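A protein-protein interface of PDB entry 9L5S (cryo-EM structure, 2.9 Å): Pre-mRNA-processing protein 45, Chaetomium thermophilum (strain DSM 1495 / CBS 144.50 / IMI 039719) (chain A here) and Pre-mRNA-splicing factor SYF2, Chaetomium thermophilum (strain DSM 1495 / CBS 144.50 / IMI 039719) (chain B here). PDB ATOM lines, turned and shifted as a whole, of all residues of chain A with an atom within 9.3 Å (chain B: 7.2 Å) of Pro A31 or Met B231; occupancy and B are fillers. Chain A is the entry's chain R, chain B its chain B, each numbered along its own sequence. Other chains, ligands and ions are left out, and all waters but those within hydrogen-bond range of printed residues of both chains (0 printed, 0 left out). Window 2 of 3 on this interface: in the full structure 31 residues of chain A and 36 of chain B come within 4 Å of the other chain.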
ATOM      1  N   GLN A  28     -33.961  19.159   3.954  1.00  0.00           N
ATOM      2  CA  GLN A  28     -34.616  18.258   3.015  1.00  0.00           C
ATOM      3  C   GLN A  28     -33.967  16.881   3.069  1.00  0.00           C
ATOM      4  O   GLN A  28     -32.740  16.759   3.008  1.00  0.00           O
ATOM      5  CB  GLN A  28     -34.550  18.832   1.600  1.00  0.00           C
ATOM      6  CG  GLN A  28     -35.038  17.888   0.516  1.00  0.00           C
ATOM      7  CD  GLN A  28     -35.732  18.615  -0.619  1.00  0.00           C
ATOM      8  OE1 GLN A  28     -36.845  19.118  -0.461  1.00  0.00           O
ATOM      9  NE2 GLN A  28     -35.075  18.677  -1.772  1.00  0.00           N
ATOM     10  N   ARG A  29     -34.794  15.847   3.198  1.00  0.00           N
ATOM     11  CA  ARG A  29     -34.296  14.487   3.346  1.00  0.00           C
ATOM     12  C   ARG A  29     -33.635  14.003   2.061  1.00  0.00           C
ATOM     13  O   ARG A  29     -33.962  14.446   0.957  1.00  0.00           O
ATOM     14  CB  ARG A  29     -35.431  13.540   3.732  1.00  0.00           C
ATOM     15  CG  ARG A  29     -36.231  13.975   4.948  1.00  0.00           C
ATOM     16  CD  ARG A  29     -35.328  14.253   6.136  1.00  0.00           C
ATOM     17  NE  ARG A  29     -35.872  15.302   6.988  1.00  0.00           N
ATOM     18  CZ  ARG A  29     -35.529  15.490   8.255  1.00  0.00           C
ATOM     19  NH1 ARG A  29     -34.643  14.711   8.854  1.00  0.00           N
ATOM     20  NH2 ARG A  29     -36.095  16.480   8.940  1.00  0.00           N
ATOM     21  N   GLY A  30     -32.684  13.085   2.218  1.00  0.00           N
ATOM     22  CA  GLY A  30     -32.011  12.494   1.092  1.00  0.00           C
ATOM     23  C   GLY A  30     -32.915  11.550   0.324  1.00  0.00           C
ATOM     24  O   GLY A  30     -33.935  11.079   0.838  1.00  0.00           O
ATOM     25  N   PRO A  31     -32.568  11.265  -0.940  1.00  0.00           N
ATOM     26  CA  PRO A  31     -31.474  11.873  -1.701  1.00  0.00           C
ATOM     27  C   PRO A  31     -31.871  13.228  -2.269  1.00  0.00           C
ATOM     28  O   PRO A  31     -33.059  13.541  -2.321  1.00  0.00           O
ATOM     29  CB  PRO A  31     -31.217  10.859  -2.829  1.00  0.00           C
ATOM     30  CG  PRO A  31     -32.113   9.673  -2.531  1.00  0.00           C
ATOM     31  CD  PRO A  31     -33.236  10.218  -1.722  1.00  0.00           C
ATOM     32  N   ARG A  32     -30.890  14.030  -2.672  1.00  0.00           N
ATOM     33  CA  ARG A  32     -31.165  15.286  -3.362  1.00  0.00           C
ATOM     34  C   ARG A  32     -31.254  14.978  -4.850  1.00  0.00           C
ATOM     35  O   ARG A  32     -30.239  14.756  -5.513  1.00  0.00           O
ATOM     36  CB  ARG A  32     -30.087  16.322  -3.067  1.00  0.00           C
ATOM     37  CG  ARG A  32     -30.480  17.737  -3.461  1.00  0.00           C
ATOM     38  CD  ARG A  32     -29.634  18.774  -2.744  1.00  0.00           C
ATOM     39  NE  ARG A  32     -28.280  18.834  -3.280  1.00  0.00           N
ATOM     40  CZ  ARG A  32     -27.871  19.708  -4.189  1.00  0.00           C
ATOM     41  NH1 ARG A  32     -28.693  20.612  -4.698  1.00  0.00           N
ATOM     42  NH2 ARG A  32     -26.607  19.676  -4.599  1.00  0.00           N
ATOM     43  N   ILE A  33     -32.474  14.951  -5.378  1.00  0.00           N
ATOM     44  CA  ILE A  33     -32.706  14.707  -6.796  1.00  0.00           C
ATOM     45  C   ILE A  33     -33.103  16.033  -7.426  1.00  0.00           C
ATOM     46  O   ILE A  33     -34.084  16.661  -7.006  1.00  0.00           O
ATOM     47  CB  ILE A  33     -33.784  13.636  -7.028  1.00  0.00           C
ATOM     48  CG1 ILE A  33     -33.375  12.297  -6.415  1.00  0.00           C
ATOM     49  CG2 ILE A  33     -34.002  13.428  -8.514  1.00  0.00           C
ATOM     50  CD1 ILE A  33     -33.987  12.011  -5.061  1.00  0.00           C
ATOM     51  N   VAL A  34     -32.346  16.460  -8.433  1.00  0.00           N
ATOM     52  CA  VAL A  34     -32.485  17.786  -9.014  1.00  0.00           C
ATOM     53  C   VAL A  34     -32.860  17.654 -10.487  1.00  0.00           C
ATOM     54  O   VAL A  34     -32.962  16.557 -11.035  1.00  0.00           O
ATOM     55  CB  VAL A  34     -31.204  18.625  -8.851  1.00  0.00           C
ATOM     56  CG1 VAL A  34     -30.865  18.789  -7.378  1.00  0.00           C
ATOM     57  CG2 VAL A  34     -30.054  17.964  -9.590  1.00  0.00           C
ATOM     58  N   THR A  42     -23.319  21.409 -10.079  1.00  0.00           N
ATOM     59  CA  THR A  42     -22.692  20.532  -9.098  1.00  0.00           C
ATOM     60  C   THR A  42     -21.484  19.818  -9.695  1.00  0.00           C
ATOM     61  O   THR A  42     -20.605  20.451 -10.282  1.00  0.00           O
ATOM     62  CB  THR A  42     -23.684  19.483  -8.561  1.00  0.00           C
ATOM     63  OG1 THR A  42     -24.190  18.698  -9.647  1.00  0.00           O
ATOM     64  CG2 THR A  42     -24.844  20.162  -7.848  1.00  0.00           C
ATOM     65  N   MET B 205     -40.474   7.822   1.085  1.00  0.00           N
ATOM     66  CA  MET B 205     -39.032   7.590   1.097  1.00  0.00           C
ATOM     67  C   MET B 205     -38.678   6.277   0.387  1.00  0.00           C
ATOM     68  O   MET B 205     -37.764   6.236  -0.446  1.00  0.00           O
ATOM     69  CB  MET B 205     -38.565   7.603   2.557  1.00  0.00           C
ATOM     70  CG  MET B 205     -37.081   7.544   2.925  1.00  0.00           C
ATOM     71  SD  MET B 205     -36.070   8.959   2.455  1.00  0.00           S
ATOM     72  CE  MET B 205     -34.439   8.218   2.414  1.00  0.00           C
ATOM     73  N   LYS B 208     -39.397   6.553  -3.390  1.00  0.00           N
ATOM     74  CA  LYS B 208     -38.409   7.437  -4.010  1.00  0.00           C
ATOM     75  C   LYS B 208     -37.082   6.715  -4.214  1.00  0.00           C
ATOM     76  O   LYS B 208     -36.494   6.792  -5.297  1.00  0.00           O
ATOM     77  CB  LYS B 208     -38.215   8.705  -3.179  1.00  0.00           C
ATOM     78  CG  LYS B 208     -37.181   9.673  -3.758  1.00  0.00           C
ATOM     79  CD  LYS B 208     -36.982  10.898  -2.875  1.00  0.00           C
ATOM     80  CE  LYS B 208     -38.072  11.931  -3.115  1.00  0.00           C
ATOM     81  NZ  LYS B 208     -37.672  13.267  -2.605  1.00  0.00           N
ATOM     82  N   LEU B 209     -36.621   5.970  -3.200  1.00  0.00           N
ATOM     83  CA  LEU B 209     -35.379   5.205  -3.352  1.00  0.00           C
ATOM     84  C   LEU B 209     -35.511   4.104  -4.397  1.00  0.00           C
ATOM     85  O   LEU B 209     -34.588   3.893  -5.192  1.00  0.00           O
ATOM     86  CB  LEU B 209     -34.925   4.618  -2.012  1.00  0.00           C
ATOM     87  CG  LEU B 209     -33.960   5.442  -1.156  1.00  0.00           C
ATOM     88  CD1 LEU B 209     -32.634   5.574  -1.877  1.00  0.00           C
ATOM     89  CD2 LEU B 209     -34.514   6.824  -0.865  1.00  0.00           C
ATOM     90  N   ILE B 212     -35.516   5.677  -7.811  1.00  0.00           N
ATOM     91  CA  ILE B 212     -34.147   6.095  -8.113  1.00  0.00           C
ATOM     92  C   ILE B 212     -33.306   4.901  -8.548  1.00  0.00           C
ATOM     93  O   ILE B 212     -32.547   4.982  -9.522  1.00  0.00           O
ATOM     94  CB  ILE B 212     -33.535   6.823  -6.900  1.00  0.00           C
ATOM     95  CG1 ILE B 212     -34.046   8.260  -6.846  1.00  0.00           C
ATOM     96  CG2 ILE B 212     -32.011   6.797  -6.934  1.00  0.00           C
ATOM     97  CD1 ILE B 212     -33.684   9.063  -8.063  1.00  0.00           C
ATOM     98  N   ASP B 222     -29.092   9.686 -13.086  1.00  0.00           N
ATOM     99  CA  ASP B 222     -27.644   9.528 -13.049  1.00  0.00           C
ATOM    100  C   ASP B 222     -27.146   9.826 -11.643  1.00  0.00           C
ATOM    101  O   ASP B 222     -27.380  10.920 -11.116  1.00  0.00           O
ATOM    102  CB  ASP B 222     -26.965  10.445 -14.069  1.00  0.00           C
ATOM    103  CG  ASP B 222     -27.527  10.275 -15.466  1.00  0.00           C
ATOM    104  OD1 ASP B 222     -28.679  10.697 -15.698  1.00  0.00           O
ATOM    105  OD2 ASP B 222     -26.818   9.720 -16.331  1.00  0.00           O
ATOM    106  N   ILE B 223     -26.472   8.847 -11.044  1.00  0.00           N
ATOM    107  CA  ILE B 223     -25.886   8.979  -9.715  1.00  0.00           C
ATOM    108  C   ILE B 223     -24.441   9.441  -9.874  1.00  0.00           C
ATOM    109  O   ILE B 223     -23.650   8.801 -10.577  1.00  0.00           O
ATOM    110  CB  ILE B 223     -25.963   7.653  -8.943  1.00  0.00           C
ATOM    111  CG1 ILE B 223     -27.384   7.416  -8.424  1.00  0.00           C
ATOM    112  CG2 ILE B 223     -24.962   7.625  -7.796  1.00  0.00           C
ATOM    113  CD1 ILE B 223     -27.598   6.035  -7.843  1.00  0.00           C
ATOM    114  N   ILE B 224     -24.101  10.561  -9.239  1.00  0.00           N
ATOM    115  CA  ILE B 224     -22.755  11.118  -9.287  1.00  0.00           C
ATOM    116  C   ILE B 224     -22.289  11.394  -7.865  1.00  0.00           C
ATOM    117  O   ILE B 224     -22.998  12.045  -7.088  1.00  0.00           O
ATOM    118  CB  ILE B 224     -22.671  12.407 -10.139  1.00  0.00           C
ATOM    119  CG1 ILE B 224     -23.019  12.157 -11.615  1.00  0.00           C
ATOM    120  CG2 ILE B 224     -21.288  13.042 -10.039  1.00  0.00           C
ATOM    121  CD1 ILE B 224     -24.481  12.292 -11.971  1.00  0.00           C
ATOM    122  N   GLU B 225     -21.107  10.891  -7.520  1.00  0.00           N
ATOM    123  CA  GLU B 225     -20.412  11.279  -6.299  1.00  0.00           C
ATOM    124  C   GLU B 225     -19.583  12.518  -6.622  1.00  0.00           C
ATOM    125  O   GLU B 225     -18.545  12.422  -7.285  1.00  0.00           O
ATOM    126  CB  GLU B 225     -19.540  10.141  -5.774  1.00  0.00           C
ATOM    127  CG  GLU B 225     -20.160   8.763  -5.938  1.00  0.00           C
ATOM    128  CD  GLU B 225     -21.374   8.563  -5.051  1.00  0.00           C
ATOM    129  OE1 GLU B 225     -21.360   9.053  -3.902  1.00  0.00           O
ATOM    130  OE2 GLU B 225     -22.342   7.917  -5.504  1.00  0.00           O
ATOM    131  N   THR B 226     -20.043  13.675  -6.156  1.00  0.00           N
ATOM    132  CA  THR B 226     -19.453  14.954  -6.529  1.00  0.00           C
ATOM    133  C   THR B 226     -18.141  15.176  -5.775  1.00  0.00           C
ATOM    134  O   THR B 226     -17.649  14.306  -5.051  1.00  0.00           O
ATOM    135  CB  THR B 226     -20.451  16.084  -6.282  1.00  0.00           C
ATOM    136  OG1 THR B 226     -19.928  17.312  -6.806  1.00  0.00           O
ATOM    137  CG2 THR B 226     -20.728  16.243  -4.791  1.00  0.00           C
ATOM    138  N   ASP B 228     -17.641  17.053  -3.283  1.00  0.00           N
ATOM    139  CA  ASP B 228     -17.894  17.130  -1.852  1.00  0.00           C
ATOM    140  C   ASP B 228     -18.194  15.770  -1.234  1.00  0.00           C
ATOM    141  O   ASP B 228     -18.457  15.697  -0.030  1.00  0.00           O
ATOM    142  CB  ASP B 228     -19.053  18.093  -1.572  1.00  0.00           C
ATOM    143  CG  ASP B 228     -18.759  19.507  -2.032  1.00  0.00           C
ATOM    144  OD1 ASP B 228     -17.650  20.007  -1.749  1.00  0.00           O
ATOM    145  OD2 ASP B 228     -19.637  20.118  -2.676  1.00  0.00           O
ATOM    146  N   GLY B 229     -18.156  14.701  -2.023  1.00  0.00           N
ATOM    147  CA  GLY B 229     -18.409  13.363  -1.518  1.00  0.00           C
ATOM    148  C   GLY B 229     -19.836  13.095  -1.090  1.00  0.00           C
ATOM    149  O   GLY B 229     -20.058  12.399  -0.091  1.00  0.00           O
ATOM    150  N   GLU B 230     -20.811  13.629  -1.821  1.00  0.00           N
ATOM    151  CA  GLU B 230     -22.220  13.375  -1.558  1.00  0.00           C
ATOM    152  C   GLU B 230     -22.878  12.856  -2.829  1.00  0.00           C
ATOM    153  O   GLU B 230     -22.559  13.306  -3.934  1.00  0.00           O
ATOM    154  CB  GLU B 230     -22.933  14.640  -1.064  1.00  0.00           C
ATOM    155  CG  GLU B 230     -24.281  14.381  -0.400  1.00  0.00           C
ATOM    156  CD  GLU B 230     -25.446  14.496  -1.363  1.00  0.00           C
ATOM    157  OE1 GLU B 230     -25.232  14.943  -2.509  1.00  0.00           O
ATOM    158  OE2 GLU B 230     -26.579  14.137  -0.974  1.00  0.00           O
ATOM    159  N   MET B 231     -23.798  11.909  -2.667  1.00  0.00           N
ATOM    160  CA  MET B 231     -24.441  11.254  -3.800  1.00  0.00           C
ATOM    161  C   MET B 231     -25.546  12.159  -4.330  1.00  0.00           C
ATOM    162  O   MET B 231     -26.561  12.370  -3.658  1.00  0.00           O
ATOM    163  CB  MET B 231     -24.976   9.887  -3.371  1.00  0.00           C
ATOM    164  CG  MET B 231     -25.625   9.030  -4.462  1.00  0.00           C
ATOM    165  SD  MET B 231     -27.349   9.383  -4.874  1.00  0.00           S
ATOM    166  CE  MET B 231     -28.178   8.740  -3.422  1.00  0.00           C
ATOM    167  N   ILE B 232     -25.353  12.699  -5.534  1.00  0.00           N
ATOM    168  CA  ILE B 232     -26.373  13.488  -6.212  1.00  0.00           C
ATOM    169  C   ILE B 232     -26.996  12.612  -7.291  1.00  0.00           C
ATOM    170  O   ILE B 232     -26.370  11.672  -7.800  1.00  0.00           O
ATOM    171  CB  ILE B 232     -25.783  14.800  -6.787  1.00  0.00           C
ATOM    172  CG1 ILE B 232     -26.878  15.845  -7.015  1.00  0.00           C
ATOM    173  CG2 ILE B 232     -24.999  14.552  -8.072  1.00  0.00           C
ATOM    174  CD1 ILE B 232     -27.411  16.454  -5.739  1.00  0.00           C
ATOM    175  N   ALA B 233     -28.254  12.895  -7.621  1.00  0.00           N
ATOM    176  CA  ALA B 233     -29.007  12.117  -8.603  1.00  0.00           C
ATOM    177  C   ALA B 233     -29.665  13.090  -9.576  1.00  0.00           C
ATOM    178  O   ALA B 233     -30.740  13.626  -9.294  1.00  0.00           O
ATOM    179  CB  ALA B 233     -30.042  11.226  -7.923  1.00  0.00           C
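SD of Met B205 lies close to O of Gly A30 (3.4 Å). The backbone NH (N) of Ala B233 sits at hydrogen-bond distance from the backbone carbonyl oxygen (O) of Arg A32, 3.4 Å away. N of Val A34 sits at hydrogen-bond distance from O of Ala B233, at 3.4 Å.
The backbone carbonyl oxygen (O) of Ile B224 is in hydrogen-bond range of the backbone NH (N) of Ile B232, 2.9 Å away.
Pro A31 touches Lys B208 (CD to CD, 3.98 Å). Leu B209 touches Pro A31 (CD2 to CD, 3.7 Å). CB of Pro A31 touches CE of Met B231, 3.8 Å away. O of Arg A32 touches CD1 of Ile B232, 3.3 Å away. Ile A33 touches Lys B208. Ile B212 touches Ile A33 (CD1 to CG1, 3.6 Å). Ala B233 touches Ile A33.
Pro A31 touches three residues of chain B. Of the printed residues of chain A, Lys B208 touches Pro A31 (3.98 Å) and Ile A33 (3.9 Å). Ile B224 touches none of the printed residues of chain A. Asp B228 touches none of the printed residues of chain A. Met B231 touches one residue of chain A. Ile B232 touches just one residue of chain A: Arg A32 (3.3 Å). Of the printed residues of chain A, Ala B233 touches Arg A32 (3.4 Å), Ile A33 (3.4 Å) and Val A34 (3.4 Å).
Of the 15 printed residues of chain B, 7 touch a printed residue of chain A. Printed residues of chain B that touch a printed residue of chain A: Met B205, Lys B208, Leu B209, Ile B212, Met B231, Ile B232 and Ala B233. Along chain B the printed residues that touch a printed residue of chain A span positions 205 to 233. Of the 8 printed residues of chain A, 5 touch a printed residue of chain B. Hydrophobic or aromatic side chains of chain A that line the printed part of chain B: Pro A31 and Ile A33. Along chain A the printed residues that touch a printed residue of chain B span positions 30 to 34. Among the printed residues, 10 pairs touch across the chains. Among the printed residues, no Asp or Glu carboxylate lies within 4 Å of a Lys or Arg side-chain nitrogen of the other chain.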
